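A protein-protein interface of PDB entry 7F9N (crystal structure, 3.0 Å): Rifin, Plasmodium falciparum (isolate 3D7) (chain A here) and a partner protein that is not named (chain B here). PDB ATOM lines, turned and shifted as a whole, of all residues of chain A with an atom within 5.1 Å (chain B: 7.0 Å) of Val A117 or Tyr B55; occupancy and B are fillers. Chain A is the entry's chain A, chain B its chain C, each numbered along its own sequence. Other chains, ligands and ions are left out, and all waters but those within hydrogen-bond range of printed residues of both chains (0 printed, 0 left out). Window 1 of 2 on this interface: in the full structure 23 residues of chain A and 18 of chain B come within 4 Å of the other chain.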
ATOM      1  N   ARG A  91      15.440 -34.261  35.458  1.00  0.00           N
ATOM      2  CA  ARG A  91      15.720 -33.520  34.238  1.00  0.00           C
ATOM      3  C   ARG A  91      17.134 -33.837  33.774  1.00  0.00           C
ATOM      4  O   ARG A  91      17.334 -34.370  32.674  1.00  0.00           O
ATOM      5  CB  ARG A  91      15.509 -32.019  34.461  1.00  0.00           C
ATOM      6  CG  ARG A  91      15.858 -31.111  33.277  1.00  0.00           C
ATOM      7  CD  ARG A  91      17.219 -30.455  33.493  1.00  0.00           C
ATOM      8  NE  ARG A  91      17.903 -30.170  32.236  1.00  0.00           N
ATOM      9  CZ  ARG A  91      18.500 -31.091  31.480  1.00  0.00           C
ATOM     10  NH1 ARG A  91      19.069 -30.749  30.336  1.00  0.00           N
ATOM     11  NH2 ARG A  91      18.536 -32.360  31.853  1.00  0.00           N
ATOM     12  N   GLY A  92      18.133 -33.546  34.631  1.00  0.00           N
ATOM     13  CA  GLY A  92      19.511 -33.912  34.347  1.00  0.00           C
ATOM     14  C   GLY A  92      19.682 -35.377  33.992  1.00  0.00           C
ATOM     15  O   GLY A  92      20.545 -35.728  33.173  1.00  0.00           O
ATOM     16  N   CYS A  95      17.538 -35.648  30.301  1.00  0.00           N
ATOM     17  CA  CYS A  95      17.957 -34.716  29.267  1.00  0.00           C
ATOM     18  C   CYS A  95      19.388 -34.233  29.497  1.00  0.00           C
ATOM     19  O   CYS A  95      19.717 -33.084  29.186  1.00  0.00           O
ATOM     20  CB  CYS A  95      16.981 -33.545  29.170  1.00  0.00           C
ATOM     21  SG  CYS A  95      15.282 -34.061  28.588  1.00  0.00           S
ATOM     22  N   GLY A  96      20.270 -35.095  30.013  1.00  0.00           N
ATOM     23  CA  GLY A  96      21.632 -34.677  30.265  1.00  0.00           C
ATOM     24  C   GLY A  96      22.468 -34.636  28.995  1.00  0.00           C
ATOM     25  O   GLY A  96      21.995 -34.917  27.893  1.00  0.00           O
ATOM     26  N   ALA A  97      23.764 -34.303  29.169  1.00  0.00           N
ATOM     27  CA  ALA A  97      24.711 -34.240  28.052  1.00  0.00           C
ATOM     28  C   ALA A  97      25.149 -35.619  27.576  1.00  0.00           C
ATOM     29  O   ALA A  97      25.717 -35.727  26.484  1.00  0.00           O
ATOM     30  CB  ALA A  97      25.936 -33.395  28.415  1.00  0.00           C
ATOM     31  N   ASN A 111      13.036 -28.043  28.859  1.00  0.00           N
ATOM     32  CA  ASN A 111      13.955 -26.995  29.295  1.00  0.00           C
ATOM     33  C   ASN A 111      13.334 -25.602  29.177  1.00  0.00           C
ATOM     34  O   ASN A 111      13.526 -24.762  30.063  1.00  0.00           O
ATOM     35  CB  ASN A 111      15.248 -27.067  28.484  1.00  0.00           C
ATOM     36  CG  ASN A 111      16.052 -28.302  28.771  1.00  0.00           C
ATOM     37  OD1 ASN A 111      16.233 -28.682  29.929  1.00  0.00           O
ATOM     38  ND2 ASN A 111      16.515 -28.964  27.708  1.00  0.00           N
ATOM     39  N   ILE A 112      12.613 -25.313  28.088  1.00  0.00           N
ATOM     40  CA  ILE A 112      11.964 -24.003  28.028  1.00  0.00           C
ATOM     41  C   ILE A 112      10.896 -23.884  29.115  1.00  0.00           C
ATOM     42  O   ILE A 112      10.796 -22.852  29.791  1.00  0.00           O
ATOM     43  CB  ILE A 112      11.353 -23.704  26.645  1.00  0.00           C
ATOM     44  CG1 ILE A 112      12.394 -23.295  25.622  1.00  0.00           C
ATOM     45  CG2 ILE A 112      10.663 -22.410  26.739  1.00  0.00           C
ATOM     46  CD1 ILE A 112      13.164 -24.394  24.997  1.00  0.00           C
ATOM     47  N   GLY A 115      12.190 -23.083  32.427  1.00  0.00           N
ATOM     48  CA  GLY A 115      12.821 -21.787  32.539  1.00  0.00           C
ATOM     49  C   GLY A 115      14.321 -21.853  32.710  1.00  0.00           C
ATOM     50  O   GLY A 115      14.912 -20.937  33.287  1.00  0.00           O
ATOM     51  N   THR A 116      14.954 -22.911  32.212  1.00  0.00           N
ATOM     52  CA  THR A 116      16.399 -23.065  32.289  1.00  0.00           C
ATOM     53  C   THR A 116      17.125 -22.664  31.015  1.00  0.00           C
ATOM     54  O   THR A 116      18.291 -22.257  31.092  1.00  0.00           O
ATOM     55  CB  THR A 116      16.758 -24.515  32.602  1.00  0.00           C
ATOM     56  OG1 THR A 116      16.410 -25.320  31.477  1.00  0.00           O
ATOM     57  CG2 THR A 116      15.993 -24.982  33.802  1.00  0.00           C
ATOM     58  N   VAL A 117      16.477 -22.760  29.851  1.00  0.00           N
ATOM     59  CA  VAL A 117      17.174 -22.719  28.574  1.00  0.00           C
ATOM     60  C   VAL A 117      16.569 -21.733  27.582  1.00  0.00           C
ATOM     61  O   VAL A 117      17.099 -21.589  26.484  1.00  0.00           O
ATOM     62  CB  VAL A 117      17.241 -24.132  27.963  1.00  0.00           C
ATOM     63  CG1 VAL A 117      17.975 -24.162  26.675  1.00  0.00           C
ATOM     64  CG2 VAL A 117      17.901 -25.047  28.909  1.00  0.00           C
ATOM     65  N   LEU A 118      15.471 -21.043  27.914  1.00  0.00           N
ATOM     66  CA  LEU A 118      15.225 -19.746  27.285  1.00  0.00           C
ATOM     67  C   LEU A 118      15.026 -19.821  25.773  1.00  0.00           C
ATOM     68  O   LEU A 118      15.986 -19.691  25.022  1.00  0.00           O
ATOM     69  CB  LEU A 118      16.414 -18.854  27.624  1.00  0.00           C
ATOM     70  CG  LEU A 118      16.627 -17.358  27.503  1.00  0.00           C
ATOM     71  CD1 LEU A 118      16.499 -16.887  26.064  1.00  0.00           C
ATOM     72  CD2 LEU A 118      15.754 -16.590  28.460  1.00  0.00           C
ATOM     73  N   ARG A 119      13.782 -19.946  25.320  1.00  0.00           N
ATOM     74  CA  ARG A 119      13.377 -20.265  23.943  1.00  0.00           C
ATOM     75  C   ARG A 119      14.418 -20.100  22.831  1.00  0.00           C
ATOM     76  O   ARG A 119      14.730 -21.068  22.127  1.00  0.00           O
ATOM     77  CB  ARG A 119      12.128 -19.451  23.588  1.00  0.00           C
ATOM     78  CG  ARG A 119      12.362 -17.962  23.364  1.00  0.00           C
ATOM     79  CD  ARG A 119      12.214 -17.123  24.641  1.00  0.00           C
ATOM     80  NE  ARG A 119      10.815 -16.999  25.129  1.00  0.00           N
ATOM     81  CZ  ARG A 119       9.781 -16.467  24.459  1.00  0.00           C
ATOM     82  NH1 ARG A 119       8.586 -16.412  25.045  1.00  0.00           N
ATOM     83  NH2 ARG A 119       9.917 -15.986  23.221  1.00  0.00           N
ATOM     84  N   GLY A 121      17.533 -19.991  22.667  1.00  0.00           N
ATOM     85  CA  GLY A 121      18.730 -20.806  22.633  1.00  0.00           C
ATOM     86  C   GLY A 121      19.620 -20.671  23.846  1.00  0.00           C
ATOM     87  O   GLY A 121      20.052 -21.684  24.393  1.00  0.00           O
ATOM     88  N   LYS A 122      19.884 -19.435  24.277  1.00  0.00           N
ATOM     89  CA  LYS A 122      20.834 -19.151  25.341  1.00  0.00           C
ATOM     90  C   LYS A 122      20.285 -19.597  26.704  1.00  0.00           C
ATOM     91  O   LYS A 122      19.112 -19.910  26.864  1.00  0.00           O
ATOM     92  CB  LYS A 122      21.210 -17.661  25.339  1.00  0.00           C
ATOM     93  CG  LYS A 122      22.491 -17.303  26.181  1.00  0.00           C
ATOM     94  CD  LYS A 122      23.633 -18.397  26.123  1.00  0.00           C
ATOM     95  CE  LYS A 122      25.017 -17.829  25.792  1.00  0.00           C
ATOM     96  NZ  LYS A 122      25.481 -16.772  26.747  1.00  0.00           N
ATOM     97  N   ALA A 123      21.176 -19.696  27.687  1.00  0.00           N
ATOM     98  CA  ALA A 123      20.794 -20.237  28.982  1.00  0.00           C
ATOM     99  C   ALA A 123      19.926 -19.241  29.704  1.00  0.00           C
ATOM    100  O   ALA A 123      20.036 -18.032  29.487  1.00  0.00           O
ATOM    101  CB  ALA A 123      22.023 -20.557  29.832  1.00  0.00           C
ATOM    102  N   ASN A 124      19.058 -19.760  30.570  1.00  0.00           N
ATOM    103  CA  ASN A 124      18.108 -18.924  31.290  1.00  0.00           C
ATOM    104  C   ASN A 124      18.488 -18.803  32.762  1.00  0.00           C
ATOM    105  O   ASN A 124      19.006 -17.753  33.165  1.00  0.00           O
ATOM    106  CB  ASN A 124      16.689 -19.442  31.124  1.00  0.00           C
ATOM    107  CG  ASN A 124      15.690 -18.503  31.702  1.00  0.00           C
ATOM    108  OD1 ASN A 124      15.965 -17.308  31.821  1.00  0.00           O
ATOM    109  ND2 ASN A 124      14.520 -19.018  32.069  1.00  0.00           N
ATOM    110  N   LEU A 125      18.241 -19.823  33.579  1.00  0.00           N
ATOM    111  CA  LEU A 125      18.865 -19.785  34.887  1.00  0.00           C
ATOM    112  C   LEU A 125      19.045 -21.198  35.415  1.00  0.00           C
ATOM    113  O   LEU A 125      18.323 -22.115  35.007  1.00  0.00           O
ATOM    114  CB  LEU A 125      18.072 -18.931  35.880  1.00  0.00           C
ATOM    115  CG  LEU A 125      16.620 -19.140  36.104  1.00  0.00           C
ATOM    116  CD1 LEU A 125      16.436 -18.598  37.480  1.00  0.00           C
ATOM    117  CD2 LEU A 125      15.830 -18.340  35.051  1.00  0.00           C
ATOM    118  N   ASP A 127      18.659 -24.095  36.562  1.00  0.00           N
ATOM    119  CA  ASP A 127      18.120 -25.433  36.784  1.00  0.00           C
ATOM    120  C   ASP A 127      17.824 -25.663  38.259  1.00  0.00           C
ATOM    121  O   ASP A 127      17.059 -26.558  38.618  1.00  0.00           O
ATOM    122  CB  ASP A 127      19.123 -26.472  36.256  1.00  0.00           C
ATOM    123  CG  ASP A 127      18.482 -27.761  35.848  1.00  0.00           C
ATOM    124  OD1 ASP A 127      17.888 -28.430  36.722  1.00  0.00           O
ATOM    125  OD2 ASP A 127      18.590 -28.122  34.656  1.00  0.00           O
ATOM    126  N   PHE B  45      27.886 -24.982  37.325  1.00  0.00           N
ATOM    127  CA  PHE B  45      28.488 -25.248  36.027  1.00  0.00           C
ATOM    128  C   PHE B  45      27.474 -26.001  35.176  1.00  0.00           C
ATOM    129  O   PHE B  45      26.691 -26.815  35.688  1.00  0.00           O
ATOM    130  CB  PHE B  45      29.794 -26.052  36.158  1.00  0.00           C
ATOM    131  CG  PHE B  45      31.024 -25.181  36.301  1.00  0.00           C
ATOM    132  CD1 PHE B  45      31.583 -24.528  35.195  1.00  0.00           C
ATOM    133  CD2 PHE B  45      31.617 -25.012  37.547  1.00  0.00           C
ATOM    134  CE1 PHE B  45      32.707 -23.730  35.339  1.00  0.00           C
ATOM    135  CE2 PHE B  45      32.734 -24.217  37.695  1.00  0.00           C
ATOM    136  CZ  PHE B  45      33.278 -23.572  36.596  1.00  0.00           C
ATOM    137  N   ARG B  46      27.483 -25.722  33.878  1.00  0.00           N
ATOM    138  CA  ARG B  46      26.637 -26.438  32.943  1.00  0.00           C
ATOM    139  C   ARG B  46      27.517 -26.969  31.822  1.00  0.00           C
ATOM    140  O   ARG B  46      28.258 -26.206  31.196  1.00  0.00           O
ATOM    141  CB  ARG B  46      25.523 -25.521  32.408  1.00  0.00           C
ATOM    142  CG  ARG B  46      24.653 -26.133  31.313  1.00  0.00           C
ATOM    143  CD  ARG B  46      23.427 -25.276  31.057  1.00  0.00           C
ATOM    144  NE  ARG B  46      22.354 -25.546  32.012  1.00  0.00           N
ATOM    145  CZ  ARG B  46      21.494 -24.626  32.428  1.00  0.00           C
ATOM    146  NH1 ARG B  46      21.626 -23.393  31.965  1.00  0.00           N
ATOM    147  NH2 ARG B  46      20.514 -24.921  33.287  1.00  0.00           N
ATOM    148  N   LEU B  47      27.475 -28.273  31.611  1.00  0.00           N
ATOM    149  CA  LEU B  47      28.093 -28.902  30.454  1.00  0.00           C
ATOM    150  C   LEU B  47      27.045 -29.044  29.356  1.00  0.00           C
ATOM    151  O   LEU B  47      26.031 -29.723  29.549  1.00  0.00           O
ATOM    152  CB  LEU B  47      28.650 -30.272  30.823  1.00  0.00           C
ATOM    153  CG  LEU B  47      29.146 -31.130  29.664  1.00  0.00           C
ATOM    154  CD1 LEU B  47      30.396 -30.531  29.035  1.00  0.00           C
ATOM    155  CD2 LEU B  47      29.368 -32.563  30.130  1.00  0.00           C
ATOM    156  N   GLU B  48      27.296 -28.436  28.202  1.00  0.00           N
ATOM    157  CA  GLU B  48      26.339 -28.381  27.106  1.00  0.00           C
ATOM    158  C   GLU B  48      26.757 -29.304  25.965  1.00  0.00           C
ATOM    159  O   GLU B  48      27.902 -29.256  25.522  1.00  0.00           O
ATOM    160  CB  GLU B  48      26.242 -26.954  26.588  1.00  0.00           C
ATOM    161  CG  GLU B  48      26.167 -25.898  27.645  1.00  0.00           C
ATOM    162  CD  GLU B  48      26.176 -24.532  27.006  1.00  0.00           C
ATOM    163  OE1 GLU B  48      27.181 -24.120  26.414  1.00  0.00           O
ATOM    164  OE2 GLU B  48      25.142 -23.875  27.025  1.00  0.00           O
ATOM    165  N   ARG B  49      25.832 -30.138  25.502  1.00  0.00           N
ATOM    166  CA  ARG B  49      25.887 -30.815  24.205  1.00  0.00           C
ATOM    167  C   ARG B  49      24.583 -30.499  23.502  1.00  0.00           C
ATOM    168  O   ARG B  49      23.535 -31.035  23.892  1.00  0.00           O
ATOM    169  CB  ARG B  49      25.998 -32.315  24.372  1.00  0.00           C
ATOM    170  CG  ARG B  49      25.713 -33.094  23.110  1.00  0.00           C
ATOM    171  CD  ARG B  49      26.013 -34.545  23.423  1.00  0.00           C
ATOM    172  NE  ARG B  49      26.353 -35.434  22.303  1.00  0.00           N
ATOM    173  CZ  ARG B  49      27.458 -35.379  21.554  1.00  0.00           C
ATOM    174  NH1 ARG B  49      27.643 -36.294  20.604  1.00  0.00           N
ATOM    175  NH2 ARG B  49      28.356 -34.404  21.709  1.00  0.00           N
ATOM    176  N   GLU B  50      24.633 -29.661  22.462  1.00  0.00           N
ATOM    177  CA  GLU B  50      23.394 -29.123  21.910  1.00  0.00           C
ATOM    178  C   GLU B  50      22.712 -28.417  23.090  1.00  0.00           C
ATOM    179  O   GLU B  50      21.980 -29.027  23.878  1.00  0.00           O
ATOM    180  CB  GLU B  50      22.584 -30.247  21.227  1.00  0.00           C
ATOM    181  CG  GLU B  50      21.130 -29.977  20.779  1.00  0.00           C
ATOM    182  CD  GLU B  50      20.803 -28.525  20.445  1.00  0.00           C
ATOM    183  OE1 GLU B  50      19.773 -28.068  20.958  1.00  0.00           O
ATOM    184  OE2 GLU B  50      21.505 -27.863  19.645  1.00  0.00           O
ATOM    185  N   SER B  51      23.008 -27.119  23.230  1.00  0.00           N
ATOM    186  CA  SER B  51      22.700 -26.360  24.440  1.00  0.00           C
ATOM    187  C   SER B  51      21.194 -26.238  24.735  1.00  0.00           C
ATOM    188  O   SER B  51      20.805 -25.956  25.880  1.00  0.00           O
ATOM    189  CB  SER B  51      23.314 -24.970  24.305  1.00  0.00           C
ATOM    190  OG  SER B  51      22.776 -24.086  25.286  1.00  0.00           O
ATOM    191  N   ARG B  52      20.339 -26.407  23.716  1.00  0.00           N
ATOM    192  CA  ARG B  52      18.895 -26.330  23.909  1.00  0.00           C
ATOM    193  C   ARG B  52      18.333 -27.594  24.581  1.00  0.00           C
ATOM    194  O   ARG B  52      17.486 -27.503  25.483  1.00  0.00           O
ATOM    195  CB  ARG B  52      18.204 -26.089  22.561  1.00  0.00           C
ATOM    196  CG  ARG B  52      18.644 -24.839  21.804  1.00  0.00           C
ATOM    197  CD  ARG B  52      18.097 -24.825  20.375  1.00  0.00           C
ATOM    198  NE  ARG B  52      17.531 -23.519  20.011  1.00  0.00           N
ATOM    199  CZ  ARG B  52      18.175 -22.590  19.304  1.00  0.00           C
ATOM    200  NH1 ARG B  52      19.404 -22.828  18.888  1.00  0.00           N
ATOM    201  NH2 ARG B  52      17.606 -21.426  19.014  1.00  0.00           N
ATOM    202  N   SER B  53      18.760 -28.784  24.154  1.00  0.00           N
ATOM    203  CA  SER B  53      18.088 -30.000  24.607  1.00  0.00           C
ATOM    204  C   SER B  53      18.823 -30.739  25.723  1.00  0.00           C
ATOM    205  O   SER B  53      18.205 -31.114  26.725  1.00  0.00           O
ATOM    206  CB  SER B  53      17.859 -30.955  23.426  1.00  0.00           C
ATOM    207  OG  SER B  53      19.060 -31.267  22.752  1.00  0.00           O
ATOM    208  N   THR B  54      20.126 -30.960  25.574  1.00  0.00           N
ATOM    209  CA  THR B  54      20.881 -31.872  26.425  1.00  0.00           C
ATOM    210  C   THR B  54      22.056 -31.139  27.077  1.00  0.00           C
ATOM    211  O   THR B  54      22.836 -30.477  26.377  1.00  0.00           O
ATOM    212  CB  THR B  54      21.345 -33.050  25.579  1.00  0.00           C
ATOM    213  OG1 THR B  54      21.731 -32.555  24.288  1.00  0.00           O
ATOM    214  CG2 THR B  54      20.224 -34.081  25.421  1.00  0.00           C
ATOM    215  N   TYR B  55      22.153 -31.231  28.414  1.00  0.00           N
ATOM    216  CA  TYR B  55      23.094 -30.475  29.249  1.00  0.00           C
ATOM    217  C   TYR B  55      22.954 -31.000  30.683  1.00  0.00           C
ATOM    218  O   TYR B  55      21.940 -31.612  31.042  1.00  0.00           O
ATOM    219  CB  TYR B  55      22.871 -28.940  29.219  1.00  0.00           C
ATOM    220  CG  TYR B  55      21.683 -28.473  30.023  1.00  0.00           C
ATOM    221  CD1 TYR B  55      20.469 -28.176  29.409  1.00  0.00           C
ATOM    222  CD2 TYR B  55      21.745 -28.389  31.406  1.00  0.00           C
ATOM    223  CE1 TYR B  55      19.333 -27.805  30.172  1.00  0.00           C
ATOM    224  CE2 TYR B  55      20.624 -28.026  32.172  1.00  0.00           C
ATOM    225  CZ  TYR B  55      19.414 -27.725  31.541  1.00  0.00           C
ATOM    226  OH  TYR B  55      18.278 -27.364  32.251  1.00  0.00           O
ATOM    227  N   ASN B  56      23.987 -30.748  31.509  1.00  0.00           N
ATOM    228  CA  ASN B  56      23.968 -31.101  32.926  1.00  0.00           C
ATOM    229  C   ASN B  56      24.475 -29.947  33.771  1.00  0.00           C
ATOM    230  O   ASN B  56      25.396 -29.220  33.382  1.00  0.00           O
ATOM    231  CB  ASN B  56      24.766 -32.359  33.193  1.00  0.00           C
ATOM    232  CG  ASN B  56      23.941 -33.609  33.004  1.00  0.00           C
ATOM    233  OD1 ASN B  56      22.745 -33.628  33.366  1.00  0.00           O
ATOM    234  ND2 ASN B  56      24.523 -34.636  32.364  1.00  0.00           N
ATOM    235  N   ASP B  57      23.804 -29.749  34.904  1.00  0.00           N
ATOM    236  CA  ASP B  57      24.109 -28.693  35.863  1.00  0.00           C
ATOM    237  C   ASP B  57      24.597 -29.325  37.152  1.00  0.00           C
ATOM    238  O   ASP B  57      23.950 -30.245  37.674  1.00  0.00           O
ATOM    239  CB  ASP B  57      22.883 -27.841  36.179  1.00  0.00           C
ATOM    240  CG  ASP B  57      22.725 -26.692  35.234  1.00  0.00           C
ATOM    241  OD1 ASP B  57      23.176 -26.814  34.083  1.00  0.00           O
ATOM    242  OD2 ASP B  57      22.178 -25.658  35.640  1.00  0.00           O
ATOM    243  N   PHE B  73      32.301 -33.707  35.069  1.00  0.00           N
ATOM    244  CA  PHE B  73      31.200 -34.552  34.634  1.00  0.00           C
ATOM    245  C   PHE B  73      31.777 -35.777  33.929  1.00  0.00           C
ATOM    246  O   PHE B  73      32.765 -35.662  33.195  1.00  0.00           O
ATOM    247  CB  PHE B  73      30.276 -33.806  33.660  1.00  0.00           C
ATOM    248  CG  PHE B  73      29.930 -32.389  34.056  1.00  0.00           C
ATOM    249  CD1 PHE B  73      30.819 -31.340  33.841  1.00  0.00           C
ATOM    250  CD2 PHE B  73      28.685 -32.107  34.597  1.00  0.00           C
ATOM    251  CE1 PHE B  73      30.484 -30.034  34.199  1.00  0.00           C
ATOM    252  CE2 PHE B  73      28.338 -30.817  34.949  1.00  0.00           C
ATOM    253  CZ  PHE B  73      29.230 -29.775  34.752  1.00  0.00           C
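O of Gly A92 lies close to OD1 of Asn B56 (3.0 Å). The backbone carbonyl oxygen (O) of Cys A95 sits close to the backbone carbonyl oxygen (O) of Ser B53, at 3.5 Å. OH of Tyr B55 sits at hydrogen-bond distance from OG1 of Thr A116, at 2.9 Å. N of Ala A97 sits close to ND2 of Asn B56 (3.3 Å). OD1 of Asn A111 lies close to OH of Tyr B55. The side-chain hydroxyl of Tyr B55 lies within hydrogen-bond range of the guanidinium group of Arg A91 (2.8 Å). OD2 of Asp A127 is in salt-bridge range of NH2 of Arg B46 (3.98 Å). ND2 of Asn A111 is in hydrogen-bond range of O of Arg B52 (2.8 Å). OD2 of Asp A127 sits at hydrogen-bond distance from OH of Tyr B55 (2.5 Å). The side-chain amide nitrogen (ND2) of Asn A111 sits at hydrogen-bond distance from the backbone carbonyl oxygen (O) of Ser B53, 2.9 Å away. The backbone carbonyl oxygen (O) of Cys A95 is in hydrogen-bond range of the backbone NH (N) of Tyr B55 (3.2 Å).
O of Lys A122 sits close to O of Val A117 (2.6 Å). The side-chain carboxylate (OD1) of Asp B57 lies within salt-bridge range of the guanidinium group (NE) of Arg B46 (2.6 Å). OG of Ser B53 sits at hydrogen-bond distance from OG1 of Thr B54, at 3.3 Å. The side-chain carboxylate (OD2) of Asp A127 lies within salt-bridge range of the guanidinium group (NE) of Arg A91 (3.2 Å). The side-chain carboxylate of Glu B50 lies close to the backbone NH of Arg B52, 3.3 Å away. The backbone carbonyl oxygen of Cys A95 lies within hydrogen-bond range of the guanidinium group of Arg A91 (2.7 Å).
Among the printed residues, merely in contact across the chains: Gly A96 with Thr B54 (3.0 Å), Gly A96 with Tyr B55 (3.2 Å), Asp A127 with Asp B57 (3.2 Å), Cys A95 with Thr B54 (3.2 Å), Ala A97 with Arg B49 (3.3 Å), Val A117 with Tyr B55 (3.4 Å), Val A117 with Ser B51 (3.4 Å), Gly A96 with Asn B56 (3.5 Å), Ala A97 with Tyr B55 (3.6 Å), Ala A123 with Arg B46 (3.6 Å), Val A117 with Arg B52 (3.6 Å), Thr A116 with Arg B46 (3.6 Å), Arg A91 with Ser B53 (3.7 Å), Gly A121 with Ser B51 (3.7 Å), Gly A121 with Arg B52 (3.8 Å), Ala A97 with Leu B47 (3.8 Å) and Leu A125 with Arg B46 (3.95 Å).
Of the printed residues of chain B, Arg A91 touches Ser B53 (3.7 Å) and Tyr B55 (2.8 Å). Of the printed residues of chain B, Gly A92 touches Asn B56. Leu A118 touches none of the printed residues of chain B. Printed residues of chain B within 4 Å of Ala A123: Arg B46 (3.6 Å). Phe B45 touches none of the printed residues of chain A. Of the printed residues of chain A, Arg B49 touches Ala A97. Printed residues of chain A within 4 Å of Ser B53: Arg A91 (3.7 Å), Cys A95 (3.5 Å) and Asn A111 (2.9 Å). Tyr B55 touches just these residues of chain A: Arg A91, Cys A95, Gly A96, Ala A97, Asn A111, Thr A116, Val A117 and Asp A127. The nearest printed residue of chain B that does not touch Leu A125 is Asp B57 (5.3 Å).
Printed residues of chain A that touch a printed residue of chain B: Arg A91, Gly A92, Cys A95, Gly A96, Ala A97, Asn A111, Thr A116, Val A117, Gly A121, Ala A123, Leu A125 and Asp A127. Hydrophobic or aromatic side chains of chain A within 4 Å of the printed part of chain B: Ala A97, Val A117 and Ala A123. Of the 14 printed residues of chain B, 10 touch a printed residue of chain A. Hydrophobic or aromatic side chains of chain B within 4 Å of the printed part of chain A: Leu B47 and Tyr B55.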
